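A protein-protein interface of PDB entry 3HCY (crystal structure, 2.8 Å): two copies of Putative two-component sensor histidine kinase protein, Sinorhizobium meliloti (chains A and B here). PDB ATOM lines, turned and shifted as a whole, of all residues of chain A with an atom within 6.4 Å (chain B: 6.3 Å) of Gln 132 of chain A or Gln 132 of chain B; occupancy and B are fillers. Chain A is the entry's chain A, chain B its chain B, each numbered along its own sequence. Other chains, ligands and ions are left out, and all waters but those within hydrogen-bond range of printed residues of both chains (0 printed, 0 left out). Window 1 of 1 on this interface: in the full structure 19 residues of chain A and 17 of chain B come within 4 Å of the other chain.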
ATOM      1  N   VAL A   7      27.208   0.501  31.665  1.00  0.00           N
ATOM      2  CA  VAL A   7      27.241   0.092  30.276  1.00  0.00           C
ATOM      3  C   VAL A   7      26.494  -1.219  30.135  1.00  0.00           C
ATOM      4  O   VAL A   7      25.803  -1.449  29.129  1.00  0.00           O
ATOM      5  CB  VAL A   7      28.641  -0.082  29.686  1.00  0.00           C
ATOM      6  CG1 VAL A   7      28.500  -0.503  28.250  1.00  0.00           C
ATOM      7  CG2 VAL A   7      29.472   1.199  29.777  1.00  0.00           C
ATOM      8  N   ALA A  10      22.658  -0.437  30.364  1.00  0.00           N
ATOM      9  CA  ALA A  10      22.272   0.228  29.097  1.00  0.00           C
ATOM     10  C   ALA A  10      22.105  -0.806  27.990  1.00  0.00           C
ATOM     11  O   ALA A  10      21.208  -0.678  27.095  1.00  0.00           O
ATOM     12  CB  ALA A  10      23.364   1.317  28.658  1.00  0.00           C
ATOM     13  N   THR A  11      22.998  -1.810  28.019  1.00  0.00           N
ATOM     14  CA  THR A  11      22.985  -2.788  26.957  1.00  0.00           C
ATOM     15  C   THR A  11      21.734  -3.619  27.121  1.00  0.00           C
ATOM     16  O   THR A  11      21.024  -3.910  26.167  1.00  0.00           O
ATOM     17  CB  THR A  11      24.169  -3.715  26.981  1.00  0.00           C
ATOM     18  OG1 THR A  11      25.381  -2.979  26.861  1.00  0.00           O
ATOM     19  CG2 THR A  11      24.082  -4.612  25.851  1.00  0.00           C
ATOM     20  N   LEU A  12      21.474  -3.996  28.359  1.00  0.00           N
ATOM     21  CA  LEU A  12      20.307  -4.765  28.676  1.00  0.00           C
ATOM     22  C   LEU A  12      19.058  -3.927  28.274  1.00  0.00           C
ATOM     23  O   LEU A  12      18.059  -4.474  27.749  1.00  0.00           O
ATOM     24  CB  LEU A  12      20.332  -5.166  30.182  1.00  0.00           C
ATOM     25  CG  LEU A  12      21.424  -6.121  30.760  1.00  0.00           C
ATOM     26  CD1 LEU A  12      21.351  -6.267  32.279  1.00  0.00           C
ATOM     27  CD2 LEU A  12      21.496  -7.530  30.053  1.00  0.00           C
ATOM     28  N   ASP A  13      19.126  -2.614  28.503  1.00  0.00           N
ATOM     29  CA  ASP A  13      18.071  -1.729  28.016  1.00  0.00           C
ATOM     30  C   ASP A  13      17.937  -1.803  26.489  1.00  0.00           C
ATOM     31  O   ASP A  13      16.818  -1.959  25.975  1.00  0.00           O
ATOM     32  CB  ASP A  13      18.280  -0.275  28.410  1.00  0.00           C
ATOM     33  CG  ASP A  13      18.184  -0.054  29.880  1.00  0.00           C
ATOM     34  OD1 ASP A  13      17.505  -0.774  30.614  1.00  0.00           O
ATOM     35  OD2 ASP A  13      18.813   0.880  30.355  1.00  0.00           O
ATOM     36  N   ALA A  14      19.061  -1.700  25.784  1.00  0.00           N
ATOM     37  CA  ALA A  14      18.988  -1.748  24.339  1.00  0.00           C
ATOM     38  C   ALA A  14      18.524  -3.144  23.924  1.00  0.00           C
ATOM     39  O   ALA A  14      17.735  -3.253  23.026  1.00  0.00           O
ATOM     40  CB  ALA A  14      20.330  -1.393  23.672  1.00  0.00           C
ATOM     41  N   ILE A  15      18.993  -4.203  24.574  1.00  0.00           N
ATOM     42  CA  ILE A  15      18.582  -5.530  24.137  1.00  0.00           C
ATOM     43  C   ILE A  15      17.056  -5.670  24.153  1.00  0.00           C
ATOM     44  O   ILE A  15      16.481  -6.202  23.202  1.00  0.00           O
ATOM     45  CB  ILE A  15      19.191  -6.669  24.957  1.00  0.00           C
ATOM     46  CG1 ILE A  15      20.632  -6.948  24.492  1.00  0.00           C
ATOM     47  CG2 ILE A  15      18.389  -7.911  24.758  1.00  0.00           C
ATOM     48  CD1 ILE A  15      21.718  -7.124  25.692  1.00  0.00           C
ATOM     49  N   LEU A 127      23.887  -8.645  16.884  1.00  0.00           N
ATOM     50  CA  LEU A 127      25.286  -8.518  16.513  1.00  0.00           C
ATOM     51  C   LEU A 127      25.777  -7.118  16.709  1.00  0.00           C
ATOM     52  O   LEU A 127      26.886  -6.880  17.225  1.00  0.00           O
ATOM     53  CB  LEU A 127      25.473  -8.878  15.052  1.00  0.00           C
ATOM     54  CG  LEU A 127      25.431 -10.382  14.830  1.00  0.00           C
ATOM     55  CD1 LEU A 127      25.080 -10.735  13.413  1.00  0.00           C
ATOM     56  CD2 LEU A 127      26.766 -10.979  15.272  1.00  0.00           C
ATOM     57  N   THR A 128      24.952  -6.174  16.287  1.00  0.00           N
ATOM     58  CA  THR A 128      25.348  -4.777  16.368  1.00  0.00           C
ATOM     59  C   THR A 128      25.611  -4.429  17.815  1.00  0.00           C
ATOM     60  O   THR A 128      26.675  -3.868  18.122  1.00  0.00           O
ATOM     61  CB  THR A 128      24.304  -3.847  15.743  1.00  0.00           C
ATOM     62  OG1 THR A 128      24.005  -4.359  14.434  1.00  0.00           O
ATOM     63  CG2 THR A 128      24.842  -2.414  15.642  1.00  0.00           C
ATOM     64  N   ILE A 129      24.700  -4.864  18.696  1.00  0.00           N
ATOM     65  CA  ILE A 129      24.844  -4.552  20.086  1.00  0.00           C
ATOM     66  C   ILE A 129      26.048  -5.254  20.725  1.00  0.00           C
ATOM     67  O   ILE A 129      26.776  -4.662  21.552  1.00  0.00           O
ATOM     68  CB  ILE A 129      23.533  -4.721  20.942  1.00  0.00           C
ATOM     69  CG1 ILE A 129      22.468  -3.745  20.554  1.00  0.00           C
ATOM     70  CG2 ILE A 129      23.680  -4.836  22.472  1.00  0.00           C
ATOM     71  CD1 ILE A 129      21.179  -4.180  21.244  1.00  0.00           C
ATOM     72  N   ALA A 130      26.269  -6.498  20.303  1.00  0.00           N
ATOM     73  CA  ALA A 130      27.414  -7.279  20.714  1.00  0.00           C
ATOM     74  C   ALA A 130      28.722  -6.580  20.318  1.00  0.00           C
ATOM     75  O   ALA A 130      29.664  -6.548  21.124  1.00  0.00           O
ATOM     76  CB  ALA A 130      27.309  -8.628  20.111  1.00  0.00           C
ATOM     77  N   ARG A 131      28.808  -5.990  19.119  1.00  0.00           N
ATOM     78  CA  ARG A 131      30.039  -5.223  18.790  1.00  0.00           C
ATOM     79  C   ARG A 131      30.191  -4.098  19.772  1.00  0.00           C
ATOM     80  O   ARG A 131      31.298  -3.818  20.255  1.00  0.00           O
ATOM     81  CB  ARG A 131      29.988  -4.500  17.470  1.00  0.00           C
ATOM     82  CG  ARG A 131      29.659  -5.286  16.254  1.00  0.00           C
ATOM     83  CD  ARG A 131      29.548  -4.293  14.981  1.00  0.00           C
ATOM     84  NE  ARG A 131      29.308  -5.044  13.732  1.00  0.00           N
ATOM     85  CZ  ARG A 131      30.263  -5.542  12.954  1.00  0.00           C
ATOM     86  NH1 ARG A 131      31.547  -5.356  13.233  1.00  0.00           N
ATOM     87  NH2 ARG A 131      29.939  -6.210  11.873  1.00  0.00           N
ATOM     88  N   GLN A 132      29.085  -3.404  20.030  1.00  0.00           N
ATOM     89  CA  GLN A 132      29.201  -2.214  20.809  1.00  0.00           C
ATOM     90  C   GLN A 132      29.605  -2.506  22.269  1.00  0.00           C
ATOM     91  O   GLN A 132      30.328  -1.685  22.922  1.00  0.00           O
ATOM     92  CB  GLN A 132      27.936  -1.393  20.754  1.00  0.00           C
ATOM     93  CG  GLN A 132      28.199   0.008  21.273  1.00  0.00           C
ATOM     94  CD  GLN A 132      27.151   1.006  20.854  1.00  0.00           C
ATOM     95  OE1 GLN A 132      26.421   0.783  19.883  1.00  0.00           O
ATOM     96  NE2 GLN A 132      27.061   2.133  21.588  1.00  0.00           N
ATOM     97  N   LEU A 133      29.149  -3.663  22.789  1.00  0.00           N
ATOM     98  CA  LEU A 133      29.621  -4.096  24.116  1.00  0.00           C
ATOM     99  C   LEU A 133      31.146  -4.364  24.042  1.00  0.00           C
ATOM    100  O   LEU A 133      31.932  -3.916  24.884  1.00  0.00           O
ATOM    101  CB  LEU A 133      28.887  -5.344  24.576  1.00  0.00           C
ATOM    102  CG  LEU A 133      29.307  -5.970  25.909  1.00  0.00           C
ATOM    103  CD1 LEU A 133      29.052  -5.007  27.065  1.00  0.00           C
ATOM    104  CD2 LEU A 133      28.604  -7.336  26.195  1.00  0.00           C
ATOM    105  N   GLY A 134      31.567  -5.084  23.017  1.00  0.00           N
ATOM    106  CA  GLY A 134      32.971  -5.368  22.896  1.00  0.00           C
ATOM    107  C   GLY A 134      33.752  -4.097  22.983  1.00  0.00           C
ATOM    108  O   GLY A 134      34.656  -3.933  23.843  1.00  0.00           O
ATOM    109  N   PHE A 135      33.396  -3.164  22.111  1.00  0.00           N
ATOM    110  CA  PHE A 135      34.137  -1.932  22.049  1.00  0.00           C
ATOM    111  C   PHE A 135      34.078  -1.117  23.313  1.00  0.00           C
ATOM    112  O   PHE A 135      35.074  -0.503  23.715  1.00  0.00           O
ATOM    113  CB  PHE A 135      33.642  -1.126  20.905  1.00  0.00           C
ATOM    114  CG  PHE A 135      34.015  -1.696  19.575  1.00  0.00           C
ATOM    115  CD1 PHE A 135      35.321  -2.022  19.283  1.00  0.00           C
ATOM    116  CD2 PHE A 135      33.066  -1.858  18.581  1.00  0.00           C
ATOM    117  CE1 PHE A 135      35.673  -2.532  18.055  1.00  0.00           C
ATOM    118  CE2 PHE A 135      33.453  -2.339  17.335  1.00  0.00           C
ATOM    119  CZ  PHE A 135      34.775  -2.677  17.089  1.00  0.00           C
ATOM    120  N   SER A 136      32.937  -1.121  23.963  1.00  0.00           N
ATOM    121  CA  SER A 136      32.809  -0.394  25.194  1.00  0.00           C
ATOM    122  C   SER A 136      33.714  -0.993  26.253  1.00  0.00           C
ATOM    123  O   SER A 136      34.410  -0.255  26.992  1.00  0.00           O
ATOM    124  CB  SER A 136      31.355  -0.381  25.653  1.00  0.00           C
ATOM    125  OG  SER A 136      30.528   0.371  24.744  1.00  0.00           O
ATOM    126  N   ILE A 137      33.754  -2.322  26.312  1.00  0.00           N
ATOM    127  CA  ILE A 137      34.692  -2.980  27.215  1.00  0.00           C
ATOM    128  C   ILE A 137      36.171  -2.712  26.812  1.00  0.00           C
ATOM    129  O   ILE A 137      36.976  -2.276  27.635  1.00  0.00           O
ATOM    130  CB  ILE A 137      34.429  -4.503  27.327  1.00  0.00           C
ATOM    131  CG1 ILE A 137      33.028  -4.783  27.911  1.00  0.00           C
ATOM    132  CG2 ILE A 137      35.481  -5.174  28.210  1.00  0.00           C
ATOM    133  CD1 ILE A 137      32.638  -6.243  27.834  1.00  0.00           C
ATOM    134  N   VAL B   7      32.805   5.408  25.941  1.00  0.00           N
ATOM    135  CA  VAL B   7      31.559   5.039  25.258  1.00  0.00           C
ATOM    136  C   VAL B   7      31.396   5.726  23.920  1.00  0.00           C
ATOM    137  O   VAL B   7      31.003   5.073  22.957  1.00  0.00           O
ATOM    138  CB  VAL B   7      30.295   5.419  26.080  1.00  0.00           C
ATOM    139  CG1 VAL B   7      29.018   5.523  25.182  1.00  0.00           C
ATOM    140  CG2 VAL B   7      30.089   4.439  27.222  1.00  0.00           C
ATOM    141  N   ALA B  10      33.785   4.040  21.562  1.00  0.00           N
ATOM    142  CA  ALA B  10      33.256   2.701  21.372  1.00  0.00           C
ATOM    143  C   ALA B  10      32.176   2.754  20.307  1.00  0.00           C
ATOM    144  O   ALA B  10      32.186   1.975  19.409  1.00  0.00           O
ATOM    145  CB  ALA B  10      32.679   2.112  22.710  1.00  0.00           C
ATOM    146  N   THR B  11      31.278   3.719  20.406  1.00  0.00           N
ATOM    147  CA  THR B  11      30.127   3.786  19.533  1.00  0.00           C
ATOM    148  C   THR B  11      30.621   4.091  18.162  1.00  0.00           C
ATOM    149  O   THR B  11      30.137   3.519  17.174  1.00  0.00           O
ATOM    150  CB  THR B  11      29.171   4.926  19.942  1.00  0.00           C
ATOM    151  OG1 THR B  11      28.653   4.700  21.273  1.00  0.00           O
ATOM    152  CG2 THR B  11      28.055   5.087  18.936  1.00  0.00           C
ATOM    153  N   ALA B  14      31.730   0.948  16.799  1.00  0.00           N
ATOM    154  CA  ALA B  14      30.597   0.131  16.428  1.00  0.00           C
ATOM    155  C   ALA B  14      29.940   0.648  15.121  1.00  0.00           C
ATOM    156  O   ALA B  14      29.643  -0.130  14.205  1.00  0.00           O
ATOM    157  CB  ALA B  14      29.598   0.074  17.584  1.00  0.00           C
ATOM    158  N   ILE B  15      29.761   1.964  15.009  1.00  0.00           N
ATOM    159  CA  ILE B  15      29.258   2.548  13.740  1.00  0.00           C
ATOM    160  C   ILE B  15      30.071   2.128  12.529  1.00  0.00           C
ATOM    161  O   ILE B  15      29.515   1.829  11.482  1.00  0.00           O
ATOM    162  CB  ILE B  15      29.223   4.072  13.773  1.00  0.00           C
ATOM    163  CG1 ILE B  15      28.069   4.530  14.690  1.00  0.00           C
ATOM    164  CG2 ILE B  15      29.122   4.622  12.356  1.00  0.00           C
ATOM    165  CD1 ILE B  15      28.168   5.980  15.180  1.00  0.00           C
ATOM    166  N   LEU B 127      19.804   2.346  14.099  1.00  0.00           N
ATOM    167  CA  LEU B 127      18.822   2.705  15.125  1.00  0.00           C
ATOM    168  C   LEU B 127      19.159   2.001  16.414  1.00  0.00           C
ATOM    169  O   LEU B 127      19.078   2.605  17.467  1.00  0.00           O
ATOM    170  CB  LEU B 127      17.395   2.356  14.676  1.00  0.00           C
ATOM    171  CG  LEU B 127      16.927   3.062  13.364  1.00  0.00           C
ATOM    172  CD1 LEU B 127      15.661   2.451  12.751  1.00  0.00           C
ATOM    173  CD2 LEU B 127      16.799   4.609  13.517  1.00  0.00           C
ATOM    174  N   THR B 128      19.548   0.732  16.326  1.00  0.00           N
ATOM    175  CA  THR B 128      20.022   0.015  17.496  1.00  0.00           C
ATOM    176  C   THR B 128      21.257   0.719  18.117  1.00  0.00           C
ATOM    177  O   THR B 128      21.325   0.925  19.305  1.00  0.00           O
ATOM    178  CB  THR B 128      20.341  -1.445  17.150  1.00  0.00           C
ATOM    179  OG1 THR B 128      19.279  -1.988  16.350  1.00  0.00           O
ATOM    180  CG2 THR B 128      20.516  -2.323  18.441  1.00  0.00           C
ATOM    181  N   ILE B 129      22.207   1.164  17.313  1.00  0.00           N
ATOM    182  CA  ILE B 129      23.343   1.912  17.892  1.00  0.00           C
ATOM    183  C   ILE B 129      22.881   3.130  18.710  1.00  0.00           C
ATOM    184  O   ILE B 129      23.359   3.308  19.833  1.00  0.00           O
ATOM    185  CB  ILE B 129      24.394   2.319  16.846  1.00  0.00           C
ATOM    186  CG1 ILE B 129      24.974   1.060  16.178  1.00  0.00           C
ATOM    187  CG2 ILE B 129      25.461   3.151  17.497  1.00  0.00           C
ATOM    188  CD1 ILE B 129      25.994   1.294  15.150  1.00  0.00           C
ATOM    189  N   ALA B 130      21.913   3.888  18.180  1.00  0.00           N
ATOM    190  CA  ALA B 130      21.484   5.167  18.743  1.00  0.00           C
ATOM    191  C   ALA B 130      20.691   4.913  20.016  1.00  0.00           C
ATOM    192  O   ALA B 130      20.660   5.712  20.985  1.00  0.00           O
ATOM    193  CB  ALA B 130      20.680   5.947  17.737  1.00  0.00           C
ATOM    194  N   ARG B 131      20.085   3.753  20.031  1.00  0.00           N
ATOM    195  CA  ARG B 131      19.332   3.311  21.184  1.00  0.00           C
ATOM    196  C   ARG B 131      20.257   3.084  22.365  1.00  0.00           C
ATOM    197  O   ARG B 131      19.981   3.477  23.498  1.00  0.00           O
ATOM    198  CB  ARG B 131      18.752   1.972  20.838  1.00  0.00           C
ATOM    199  CG  ARG B 131      17.310   1.797  21.001  1.00  0.00           C
ATOM    200  CD  ARG B 131      16.991   0.267  20.911  1.00  0.00           C
ATOM    201  NE  ARG B 131      16.216  -0.011  19.719  1.00  0.00           N
ATOM    202  CZ  ARG B 131      14.916   0.215  19.633  1.00  0.00           C
ATOM    203  NH1 ARG B 131      14.249   0.701  20.685  1.00  0.00           N
ATOM    204  NH2 ARG B 131      14.294  -0.042  18.487  1.00  0.00           N
ATOM    205  N   GLN B 132      21.367   2.414  22.091  1.00  0.00           N
ATOM    206  CA  GLN B 132      22.290   2.048  23.128  1.00  0.00           C
ATOM    207  C   GLN B 132      23.033   3.262  23.688  1.00  0.00           C
ATOM    208  O   GLN B 132      23.360   3.299  24.887  1.00  0.00           O
ATOM    209  CB  GLN B 132      23.302   1.070  22.568  1.00  0.00           C
ATOM    210  CG  GLN B 132      24.158   0.413  23.622  1.00  0.00           C
ATOM    211  CD  GLN B 132      24.222  -1.095  23.434  1.00  0.00           C
ATOM    212  OE1 GLN B 132      25.135  -1.657  22.777  1.00  0.00           O
ATOM    213  NE2 GLN B 132      23.222  -1.777  23.998  1.00  0.00           N
ATOM    214  N   LEU B 133      23.359   4.222  22.813  1.00  0.00           N
ATOM    215  CA  LEU B 133      24.130   5.396  23.214  1.00  0.00           C
ATOM    216  C   LEU B 133      23.248   6.165  24.149  1.00  0.00           C
ATOM    217  O   LEU B 133      23.657   6.523  25.267  1.00  0.00           O
ATOM    218  CB  LEU B 133      24.425   6.265  22.006  1.00  0.00           C
ATOM    219  CG  LEU B 133      25.163   7.571  22.259  1.00  0.00           C
ATOM    220  CD1 LEU B 133      26.514   7.213  22.810  1.00  0.00           C
ATOM    221  CD2 LEU B 133      25.252   8.394  21.009  1.00  0.00           C
ATOM    222  N   GLY B 134      22.004   6.360  23.678  1.00  0.00           N
ATOM    223  CA  GLY B 134      20.949   7.027  24.448  1.00  0.00           C
ATOM    224  C   GLY B 134      20.920   6.467  25.850  1.00  0.00           C
ATOM    225  O   GLY B 134      21.053   7.242  26.818  1.00  0.00           O
ATOM    226  N   PHE B 135      20.830   5.127  25.973  1.00  0.00           N
ATOM    227  CA  PHE B 135      20.752   4.517  27.306  1.00  0.00           C
ATOM    228  C   PHE B 135      22.067   4.607  28.062  1.00  0.00           C
ATOM    229  O   PHE B 135      22.090   4.883  29.258  1.00  0.00           O
ATOM    230  CB  PHE B 135      20.341   3.073  27.220  1.00  0.00           C
ATOM    231  CG  PHE B 135      18.903   2.876  26.918  1.00  0.00           C
ATOM    232  CD1 PHE B 135      17.932   3.399  27.744  1.00  0.00           C
ATOM    233  CD2 PHE B 135      18.498   2.110  25.817  1.00  0.00           C
ATOM    234  CE1 PHE B 135      16.606   3.209  27.456  1.00  0.00           C
ATOM    235  CE2 PHE B 135      17.150   1.904  25.544  1.00  0.00           C
ATOM    236  CZ  PHE B 135      16.222   2.468  26.351  1.00  0.00           C
ATOM    237  N   SER B 136      23.167   4.367  27.372  1.00  0.00           N
ATOM    238  CA  SER B 136      24.472   4.616  27.980  1.00  0.00           C
ATOM    239  C   SER B 136      24.558   6.017  28.621  1.00  0.00           C
ATOM    240  O   SER B 136      24.814   6.121  29.824  1.00  0.00           O
ATOM    241  CB  SER B 136      25.627   4.315  26.995  1.00  0.00           C
ATOM    242  OG  SER B 136      25.672   2.901  26.631  1.00  0.00           O
ATOM    243  N   ILE B 137      24.285   7.073  27.844  1.00  0.00           N
ATOM    244  CA  ILE B 137      24.291   8.435  28.403  1.00  0.00           C
ATOM    245  C   ILE B 137      23.263   8.530  29.547  1.00  0.00           C
ATOM    246  O   ILE B 137      23.581   9.073  30.628  1.00  0.00           O
ATOM    247  CB  ILE B 137      23.912   9.515  27.390  1.00  0.00           C
ATOM    248  CG1 ILE B 137      24.911   9.587  26.223  1.00  0.00           C
ATOM    249  CG2 ILE B 137      23.824  10.866  28.075  1.00  0.00           C
ATOM    250  CD1 ILE B 137      24.277  10.222  24.992  1.00  0.00           C
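OG1 of Thr 11 of chain B sits at hydrogen-bond distance from NE2 of Gln 132 of chain A, at 3.0 Å.
Ala 10 of chain A touches Phe 135 of chain B, and with the chains exchanged Phe 135 of chain A touches Ala 10 of chain B. Thr 11 of chain A touches Gln 132 of chain B, and with the chains exchanged Gln 132 of chain A touches Thr 11 of chain B. Ala 14 of chain A touches Gln 132 of chain B, and with the chains exchanged Gln 132 of chain A touches Ala 14 of chain B. Ala 14 of chain A touches Phe 135 of chain B, and with the chains exchanged Phe 135 of chain A touches Ala 14 of chain B. 16 positions are printed for both chains. Of the 17 pairs that touch across the chains among the printed residues, 15 have their exchanged pair printed and touching as well.
Of the printed residues of chain B, Thr 11 of chain A touches Gln 132 (3.1 Å). Of the printed residues of chain B, Ala 14 of chain A touches Gln 132 (2.9 Å) and Phe 135 (3.9 Å). Of the printed residues of chain B, Thr 128 of chain A touches Ile 129. Gln 132 of chain A touches four residues of chain B. Of the printed residues of chain A, Ala 10 of chain B touches Phe 135 (3.6 Å) and Ser 136 (3.4 Å). Ile 15 of chain B touches none of the printed residues of chain A. Gln 132 of chain B touches just these residues of chain A: Ala 10 (3.9 Å), Thr 11 (3.1 Å), Ala 14 (2.9 Å), Ile 129 (3.4 Å) and Gln 132 (3.5 Å). Gly 134 of chain B touches none of the printed residues of chain A. Printed residues of chain A within 4 Å of Phe 135 of chain B: Ala 10 (3.6 Å), Asp 13 (3.5 Å) and Ala 14 (3.9 Å). The nearest residue of chain B that does not touch Gln 132 of chain A is Leu 133 of chain B (4.4 Å). The nearest printed residue of chain B that does not touch Ala 10 of chain A is Arg 131 of chain B (5.6 Å).
The side-chain hydroxyl (OG1) of Thr 11 of chain A lies within hydrogen-bond range of the backbone carbonyl oxygen (O) of Val 7 of chain A (2.8 Å). The side-chain hydroxyl of Thr 11 of chain B is in hydrogen-bond range of the backbone carbonyl oxygen of Val 7 of chain B (2.9 Å). The backbone carbonyl oxygen (O) of Gln 132 of chain B sits at hydrogen-bond distance from the side-chain hydroxyl (OG) of Ser 136 of chain B (2.9 Å). O of Gln 132 of chain A sits at hydrogen-bond distance from OG of Ser 136 of chain A, at 2.8 Å.
Of the 16 printed residues of chain B, 8 touch a printed residue of chain A. Hydrophobic or aromatic side chains of chain B within 4 Å of the printed part of chain A: Ala 10, Ala 14, Ile 129 and Phe 135. Among the printed residues, 17 pairs touch across the chains. Among the printed residues, no Asp or Glu carboxylate lies within 4 Å of a Lys or Arg side-chain nitrogen of the other chain.
Among the printed residues, pairs that only touch across the chains: Ala 14 of chain A with Gln 132 of chain B (2.9 Å), Thr 11 of chain A with Gln 132 of chain B (3.1 Å), Ile 129 of chain A with Thr 128 of chain B (3.2 Å), Ala 10 of chain A with Ser 136 of chain B (3.3 Å), Ser 136 of chain A with Ala 10 of chain B (3.4 Å), Ile 129 of chain A with Gln 132 of chain B (3.4 Å), Gln 132 of chain A with Gln 132 of chain B (3.5 Å), Gln 132 of chain A with Ile 129 of chain B (3.5 Å), Thr 128 of chain A with Ile 129 of chain B (3.5 Å), Asp 13 of chain A with Phe 135 of chain B (3.5 Å), Phe 135 of chain A with Ala 10 of chain B (3.6 Å), Phe 135 of chain A with Ala 14 of chain B (3.6 Å), Ala 10 of chain A with Phe 135 of chain B (3.6 Å), Ala 14 of chain A with Phe 135 of chain B (3.9 Å), Ala 10 of chain A with Gln 132 of chain B (3.9 Å) and Gln 132 of chain A with Ala 14 of chain B (3.9 Å).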
